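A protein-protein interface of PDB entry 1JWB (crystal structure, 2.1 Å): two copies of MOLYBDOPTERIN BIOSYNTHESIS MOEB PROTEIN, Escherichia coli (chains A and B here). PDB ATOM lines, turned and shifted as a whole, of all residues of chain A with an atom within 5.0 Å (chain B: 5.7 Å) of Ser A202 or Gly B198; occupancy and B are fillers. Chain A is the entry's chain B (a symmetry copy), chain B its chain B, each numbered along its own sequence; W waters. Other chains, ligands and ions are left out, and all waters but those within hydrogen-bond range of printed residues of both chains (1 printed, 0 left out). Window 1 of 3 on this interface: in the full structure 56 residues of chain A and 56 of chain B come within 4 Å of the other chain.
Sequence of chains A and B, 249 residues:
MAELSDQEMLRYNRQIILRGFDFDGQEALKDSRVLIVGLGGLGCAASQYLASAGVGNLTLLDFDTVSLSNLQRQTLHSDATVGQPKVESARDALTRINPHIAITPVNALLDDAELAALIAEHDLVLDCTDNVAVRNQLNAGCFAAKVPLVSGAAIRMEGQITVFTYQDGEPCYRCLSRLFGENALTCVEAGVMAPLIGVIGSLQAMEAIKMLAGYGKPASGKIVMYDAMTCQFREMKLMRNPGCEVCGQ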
ATOM      1  N   ALA A  45      24.151  25.141 -30.971  1.00  0.00           N
ATOM      2  CA  ALA A  45      24.511  24.901 -29.567  1.00  0.00           C
ATOM      3  C   ALA A  45      25.929  24.385 -29.478  1.00  0.00           C
ATOM      4  O   ALA A  45      26.711  24.872 -28.664  1.00  0.00           O
ATOM      5  CB  ALA A  45      23.554  23.915 -28.900  1.00  0.00           C
ATOM      6  N   ALA A  46      26.303  23.504 -30.397  1.00  0.00           N
ATOM      7  CA  ALA A  46      27.626  22.903 -30.314  1.00  0.00           C
ATOM      8  C   ALA A  46      28.736  23.838 -30.825  1.00  0.00           C
ATOM      9  O   ALA A  46      29.806  23.953 -30.201  1.00  0.00           O
ATOM     10  CB  ALA A  46      27.707  21.524 -31.062  1.00  0.00           C
ATOM     11  N   TYR A  49      30.205  26.635 -28.502  1.00  0.00           N
ATOM     12  CA  TYR A  49      31.251  26.267 -27.578  1.00  0.00           C
ATOM     13  C   TYR A  49      32.476  25.699 -28.204  1.00  0.00           C
ATOM     14  O   TYR A  49      33.552  25.782 -27.625  1.00  0.00           O
ATOM     15  CB  TYR A  49      30.731  25.281 -26.539  1.00  0.00           C
ATOM     16  CG  TYR A  49      29.718  25.906 -25.706  1.00  0.00           C
ATOM     17  CD1 TYR A  49      28.378  25.549 -25.820  1.00  0.00           C
ATOM     18  CD2 TYR A  49      30.053  26.944 -24.861  1.00  0.00           C
ATOM     19  CE1 TYR A  49      27.419  26.170 -25.090  1.00  0.00           C
ATOM     20  CE2 TYR A  49      29.054  27.610 -24.115  1.00  0.00           C
ATOM     21  CZ  TYR A  49      27.749  27.201 -24.217  1.00  0.00           C
ATOM     22  OH  TYR A  49      26.766  27.839 -23.449  1.00  0.00           O
ATOM     23  N   ILE A 197      18.367  21.192 -27.073  1.00  0.00           N
ATOM     24  CA  ILE A 197      19.425  21.332 -28.046  1.00  0.00           C
ATOM     25  C   ILE A 197      20.673  21.835 -27.394  1.00  0.00           C
ATOM     26  O   ILE A 197      21.760  21.515 -27.803  1.00  0.00           O
ATOM     27  CB  ILE A 197      18.902  22.284 -29.176  1.00  0.00           C
ATOM     28  CG1 ILE A 197      18.858  21.512 -30.446  1.00  0.00           C
ATOM     29  CG2 ILE A 197      19.633  23.583 -29.238  1.00  0.00           C
ATOM     30  CD1 ILE A 197      17.789  20.509 -30.354  1.00  0.00           C
ATOM     31  N   GLY A 198      20.507  22.660 -26.396  1.00  0.00           N
ATOM     32  CA  GLY A 198      21.608  23.165 -25.649  1.00  0.00           C
ATOM     33  C   GLY A 198      22.313  22.055 -24.934  1.00  0.00           C
ATOM     34  O   GLY A 198      23.510  21.959 -25.009  1.00  0.00           O
ATOM     35  N   VAL A 199      21.558  21.199 -24.282  1.00  0.00           N
ATOM     36  CA  VAL A 199      22.164  20.104 -23.555  1.00  0.00           C
ATOM     37  C   VAL A 199      22.933  19.216 -24.520  1.00  0.00           C
ATOM     38  O   VAL A 199      24.113  18.947 -24.317  1.00  0.00           O
ATOM     39  CB  VAL A 199      21.096  19.268 -22.818  1.00  0.00           C
ATOM     40  CG1 VAL A 199      21.684  18.071 -22.149  1.00  0.00           C
ATOM     41  CG2 VAL A 199      20.323  20.113 -21.806  1.00  0.00           C
ATOM     42  N   ILE A 200      22.263  18.713 -25.541  1.00  0.00           N
ATOM     43  CA  ILE A 200      22.914  17.761 -26.391  1.00  0.00           C
ATOM     44  C   ILE A 200      24.044  18.391 -27.210  1.00  0.00           C
ATOM     45  O   ILE A 200      25.094  17.800 -27.430  1.00  0.00           O
ATOM     46  CB  ILE A 200      21.876  17.081 -27.325  1.00  0.00           C
ATOM     47  CG1 ILE A 200      20.892  16.243 -26.536  1.00  0.00           C
ATOM     48  CG2 ILE A 200      22.589  16.184 -28.291  1.00  0.00           C
ATOM     49  CD1 ILE A 200      21.589  15.261 -25.569  1.00  0.00           C
ATOM     50  N   GLY A 201      23.819  19.615 -27.686  1.00  0.00           N
ATOM     51  CA  GLY A 201      24.834  20.319 -28.486  1.00  0.00           C
ATOM     52  C   GLY A 201      26.081  20.578 -27.659  1.00  0.00           C
ATOM     53  O   GLY A 201      27.223  20.453 -28.127  1.00  0.00           O
ATOM     54  N   SER A 202      25.875  20.934 -26.398  1.00  0.00           N
ATOM     55  CA  SER A 202      27.012  21.190 -25.537  1.00  0.00           C
ATOM     56  C   SER A 202      27.736  19.895 -25.238  1.00  0.00           C
ATOM     57  O   SER A 202      28.969  19.898 -25.189  1.00  0.00           O
ATOM     58  CB  SER A 202      26.602  21.910 -24.269  1.00  0.00           C
ATOM     59  OG  SER A 202      25.822  23.051 -24.561  1.00  0.00           O
ATOM     60  N   LEU A 203      26.995  18.798 -25.086  1.00  0.00           N
ATOM     61  CA  LEU A 203      27.608  17.494 -24.878  1.00  0.00           C
ATOM     62  C   LEU A 203      28.416  17.144 -26.120  1.00  0.00           C
ATOM     63  O   LEU A 203      29.500  16.632 -26.002  1.00  0.00           O
ATOM     64  CB  LEU A 203      26.563  16.384 -24.633  1.00  0.00           C
ATOM     65  CG  LEU A 203      25.887  16.353 -23.260  1.00  0.00           C
ATOM     66  CD1 LEU A 203      24.694  15.442 -23.237  1.00  0.00           C
ATOM     67  CD2 LEU A 203      26.893  16.050 -22.106  1.00  0.00           C
ATOM     68  N   GLN A 204      27.891  17.412 -27.310  1.00  0.00           N
ATOM     69  CA  GLN A 204      28.664  17.190 -28.524  1.00  0.00           C
ATOM     70  C   GLN A 204      29.936  18.024 -28.460  1.00  0.00           C
ATOM     71  O   GLN A 204      31.025  17.528 -28.711  1.00  0.00           O
ATOM     72  CB  GLN A 204      27.872  17.561 -29.771  1.00  0.00           C
ATOM     73  CG  GLN A 204      26.676  16.617 -30.100  1.00  0.00           C
ATOM     74  CD  GLN A 204      26.097  16.842 -31.506  1.00  0.00           C
ATOM     75  OE1 GLN A 204      25.052  17.469 -31.626  1.00  0.00           O
ATOM     76  NE2 GLN A 204      26.748  16.294 -32.555  1.00  0.00           N
ATOM     77  N   ALA A 205      29.828  19.295 -28.132  1.00  0.00           N
ATOM     78  CA  ALA A 205      31.038  20.103 -28.076  1.00  0.00           C
ATOM     79  C   ALA A 205      32.050  19.467 -27.114  1.00  0.00           C
ATOM     80  O   ALA A 205      33.256  19.390 -27.402  1.00  0.00           O
ATOM     81  CB  ALA A 205      30.740  21.502 -27.653  1.00  0.00           C
ATOM     82  N   MET A 206      31.547  19.006 -25.957  1.00  0.00           N
ATOM     83  CA  MET A 206      32.407  18.451 -24.945  1.00  0.00           C
ATOM     84  C   MET A 206      33.162  17.211 -25.441  1.00  0.00           C
ATOM     85  O   MET A 206      34.372  17.129 -25.294  1.00  0.00           O
ATOM     86  CB  MET A 206      31.624  18.118 -23.692  1.00  0.00           C
ATOM     87  CG  MET A 206      32.480  17.537 -22.533  1.00  0.00           C
ATOM     88  SD  MET A 206      33.668  18.660 -21.983  1.00  0.00           S
ATOM     89  CE  MET A 206      32.689  19.610 -20.795  1.00  0.00           C
ATOM     90  N   GLY B  41      29.245  32.111 -16.910  1.00  0.00           N
ATOM     91  CA  GLY B  41      29.124  30.926 -17.731  1.00  0.00           C
ATOM     92  C   GLY B  41      27.770  30.274 -17.660  1.00  0.00           C
ATOM     93  O   GLY B  41      27.095  30.062 -18.701  1.00  0.00           O
ATOM     94  N   ALA B  45      24.693  30.587 -20.567  1.00  0.00           N
ATOM     95  CA  ALA B  45      24.197  29.354 -21.193  1.00  0.00           C
ATOM     96  C   ALA B  45      22.717  29.199 -20.926  1.00  0.00           C
ATOM     97  O   ALA B  45      21.954  28.912 -21.847  1.00  0.00           O
ATOM     98  CB  ALA B  45      24.949  28.124 -20.689  1.00  0.00           C
ATOM     99  N   ALA B 194      34.826  24.852 -21.341  1.00  0.00           N
ATOM    100  CA  ALA B 194      33.738  25.654 -21.857  1.00  0.00           C
ATOM    101  C   ALA B 194      32.361  24.997 -21.969  1.00  0.00           C
ATOM    102  O   ALA B 194      31.387  25.475 -21.380  1.00  0.00           O
ATOM    103  CB  ALA B 194      34.114  26.356 -23.091  1.00  0.00           C
ATOM    104  N   PRO B 195      32.240  23.950 -22.740  1.00  0.00           N
ATOM    105  CA  PRO B 195      30.948  23.308 -22.920  1.00  0.00           C
ATOM    106  C   PRO B 195      30.307  22.812 -21.630  1.00  0.00           C
ATOM    107  O   PRO B 195      29.168  22.529 -21.692  1.00  0.00           O
ATOM    108  CB  PRO B 195      31.273  22.086 -23.797  1.00  0.00           C
ATOM    109  CG  PRO B 195      32.600  22.128 -24.157  1.00  0.00           C
ATOM    110  CD  PRO B 195      33.257  23.334 -23.581  1.00  0.00           C
ATOM    111  N   LEU B 196      31.035  22.630 -20.546  1.00  0.00           N
ATOM    112  CA  LEU B 196      30.426  22.146 -19.349  1.00  0.00           C
ATOM    113  C   LEU B 196      29.266  23.095 -18.978  1.00  0.00           C
ATOM    114  O   LEU B 196      28.166  22.692 -18.573  1.00  0.00           O
ATOM    115  CB  LEU B 196      31.506  22.115 -18.248  1.00  0.00           C
ATOM    116  CG  LEU B 196      31.097  21.743 -16.839  1.00  0.00           C
ATOM    117  CD1 LEU B 196      30.494  20.380 -16.876  1.00  0.00           C
ATOM    118  CD2 LEU B 196      32.201  21.803 -15.824  1.00  0.00           C
ATOM    119  N   ILE B 197      29.542  24.376 -19.096  1.00  0.00           N
ATOM    120  CA  ILE B 197      28.591  25.403 -18.740  1.00  0.00           C
ATOM    121  C   ILE B 197      27.382  25.325 -19.617  1.00  0.00           C
ATOM    122  O   ILE B 197      26.293  25.640 -19.205  1.00  0.00           O
ATOM    123  CB  ILE B 197      29.329  26.783 -18.842  1.00  0.00           C
ATOM    124  CG1 ILE B 197      29.357  27.392 -17.486  1.00  0.00           C
ATOM    125  CG2 ILE B 197      28.797  27.657 -19.928  1.00  0.00           C
ATOM    126  CD1 ILE B 197      30.261  26.608 -16.634  1.00  0.00           C
ATOM    127  N   GLY B 198      27.588  24.938 -20.847  1.00  0.00           N
ATOM    128  CA  GLY B 198      26.518  24.763 -21.767  1.00  0.00           C
ATOM    129  C   GLY B 198      25.608  23.663 -21.315  1.00  0.00           C
ATOM    130  O   GLY B 198      24.419  23.843 -21.285  1.00  0.00           O
ATOM    131  N   VAL B 199      26.181  22.547 -20.925  1.00  0.00           N
ATOM    132  CA  VAL B 199      25.371  21.431 -20.484  1.00  0.00           C
ATOM    133  C   VAL B 199      24.559  21.841 -19.267  1.00  0.00           C
ATOM    134  O   VAL B 199      23.341  21.695 -19.250  1.00  0.00           O
ATOM    135  CB  VAL B 199      26.250  20.210 -20.135  1.00  0.00           C
ATOM    136  CG1 VAL B 199      25.448  19.083 -19.575  1.00  0.00           C
ATOM    137  CG2 VAL B 199      27.057  19.737 -21.343  1.00  0.00           C
ATOM    138  N   ILE B 200      25.225  22.305 -18.225  1.00  0.00           N
ATOM    139  CA  ILE B 200      24.511  22.569 -17.011  1.00  0.00           C
ATOM    140  C   ILE B 200      23.549  23.752 -17.150  1.00  0.00           C
ATOM    141  O   ILE B 200      22.443  23.755 -16.620  1.00  0.00           O
ATOM    142  CB  ILE B 200      25.508  22.811 -15.846  1.00  0.00           C
ATOM    143  CG1 ILE B 200      26.299  21.558 -15.531  1.00  0.00           C
ATOM    144  CG2 ILE B 200      24.750  23.209 -14.616  1.00  0.00           C
ATOM    145  CD1 ILE B 200      25.397  20.321 -15.325  1.00  0.00           C
ATOM    146  N   GLY B 201      23.981  24.787 -17.868  1.00  0.00           N
ATOM    147  CA  GLY B 201      23.141  25.979 -18.069  1.00  0.00           C
ATOM    148  C   GLY B 201      21.884  25.622 -18.845  1.00  0.00           C
ATOM    149  O   GLY B 201      20.776  26.100 -18.563  1.00  0.00           O
ATOM    150  N   SER B 202      22.043  24.755 -19.835  1.00  0.00           N
ATOM    151  CA  SER B 202      20.893  24.352 -20.619  1.00  0.00           C
ATOM    152  C   SER B 202      19.970  23.494 -19.780  1.00  0.00           C
ATOM    153  O   SER B 202      18.750  23.632 -19.904  1.00  0.00           O
ATOM    154  CB  SER B 202      21.305  23.652 -21.897  1.00  0.00           C
ATOM    155  OG  SER B 202      22.261  24.411 -22.609  1.00  0.00           O
ATOM    156  N   LEU B 203      20.533  22.657 -18.911  1.00  0.00           N
ATOM    157  CA  LEU B 203      19.727  21.852 -18.004  1.00  0.00           C
ATOM    158  C   LEU B 203      18.972  22.793 -17.075  1.00  0.00           C
ATOM    159  O   LEU B 203      17.821  22.568 -16.804  1.00  0.00           O
ATOM    160  CB  LEU B 203      20.580  20.888 -17.153  1.00  0.00           C
ATOM    161  CG  LEU B 203      21.138  19.647 -17.855  1.00  0.00           C
ATOM    162  CD1 LEU B 203      22.183  18.953 -17.029  1.00  0.00           C
ATOM    163  CD2 LEU B 203      20.014  18.676 -18.336  1.00  0.00           C
ATOM    164  N   TYR B 226      27.091  15.517 -13.408  1.00  0.00           N
ATOM    165  CA  TYR B 226      27.562  15.222 -14.744  1.00  0.00           C
ATOM    166  C   TYR B 226      29.047  15.235 -14.647  1.00  0.00           C
ATOM    167  O   TYR B 226      29.668  16.245 -14.254  1.00  0.00           O
ATOM    168  CB  TYR B 226      27.130  16.334 -15.701  1.00  0.00           C
ATOM    169  CG  TYR B 226      27.837  16.403 -17.018  1.00  0.00           C
ATOM    170  CD1 TYR B 226      28.120  15.262 -17.756  1.00  0.00           C
ATOM    171  CD2 TYR B 226      28.204  17.624 -17.543  1.00  0.00           C
ATOM    172  CE1 TYR B 226      28.737  15.346 -18.964  1.00  0.00           C
ATOM    173  CE2 TYR B 226      28.832  17.710 -18.742  1.00  0.00           C
ATOM    174  CZ  TYR B 226      29.098  16.583 -19.458  1.00  0.00           C
ATOM    175  OH  TYR B 226      29.790  16.688 -20.641  1.00  0.00           O
HETATM  176  O   HOH W   1      27.871  30.646 -21.904  1.00  0.00           O
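Gly A198 touches Ser B202, and with the chains exchanged Ser A202 touches Gly B198.
Val A199 touches Ser B202, and with the chains exchanged Ser A202 touches Val B199.
Val A199 touches Leu B203, and with the chains exchanged Leu A203 touches Val B199.
Of the 14 pairs that touch across the chains among the printed residues, 6 have their exchanged pair printed and touching as well.
Hydrophobic or aromatic side chains of chain B that line the printed part of chain A: Ala B45, Pro B195, Leu B196, Val B199, Leu B203 and Tyr B226.
Hydrophobic or aromatic side chains of chain A within 4 Å of the printed part of chain B: Tyr A49, Val A199, Leu A203, Ala A205 and Met A206.
Among the printed residues, pairs that only touch across the chains: Leu A203 with Tyr B226 (3.3 Å), Ser A202 with Gly B198 (3.3 Å), Gly A198 with Ser B202 (3.3 Å), Tyr A49 with Ala B45 (3.3 Å), Met A206 with Tyr B226 (3.4 Å), Ser A202 with Val B199 (3.4 Å), Val A199 with Ser B202 (3.4 Å), Met A206 with Leu B196 (3.5 Å), Ser A202 with Pro B195 (3.5 Å), Tyr A49 with Gly B198 (3.5 Å), Met A206 with Pro B195 (3.8 Å), Val A199 with Leu B203 (3.8 Å), Leu A203 with Val B199 (3.8 Å) and Ala A205 with Pro B195 (3.9 Å).
Water W1 lies within hydrogen-bond range of O of Gly B41 (3.3 Å), OH of Tyr A49 (3.4 Å) and N of Ala B45 (3.4 Å).
The backbone carbonyl oxygen (O) of Gly B198 sits at hydrogen-bond distance from the side-chain hydroxyl (OG) of Ser B202 (2.6 Å).
The backbone carbonyl oxygen (O) of Gly A198 sits at hydrogen-bond distance from the side-chain hydroxyl (OG) of Ser A202.
Ser A202 touches three residues of chain B.
Gly B198 touches just these residues of chain A: Tyr A49 (3.5 Å) and Ser A202 (3.3 Å).
Of the printed residues of chain A, Pro B195 touches Ser A202, Ala A205 and Met A206.
Of the printed residues of chain B, Gly A198 touches Ser B202 (3.3 Å).
The nearest residue of chain B that does not touch Ser A202 is Ser B202 (4.3 Å).
The nearest residue of chain A that does not touch Gly B198 is Gly A198 (4.3 Å).
The nearest printed residue of chain B that does not touch Ala A205 is Ala B194 (6.9 Å).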
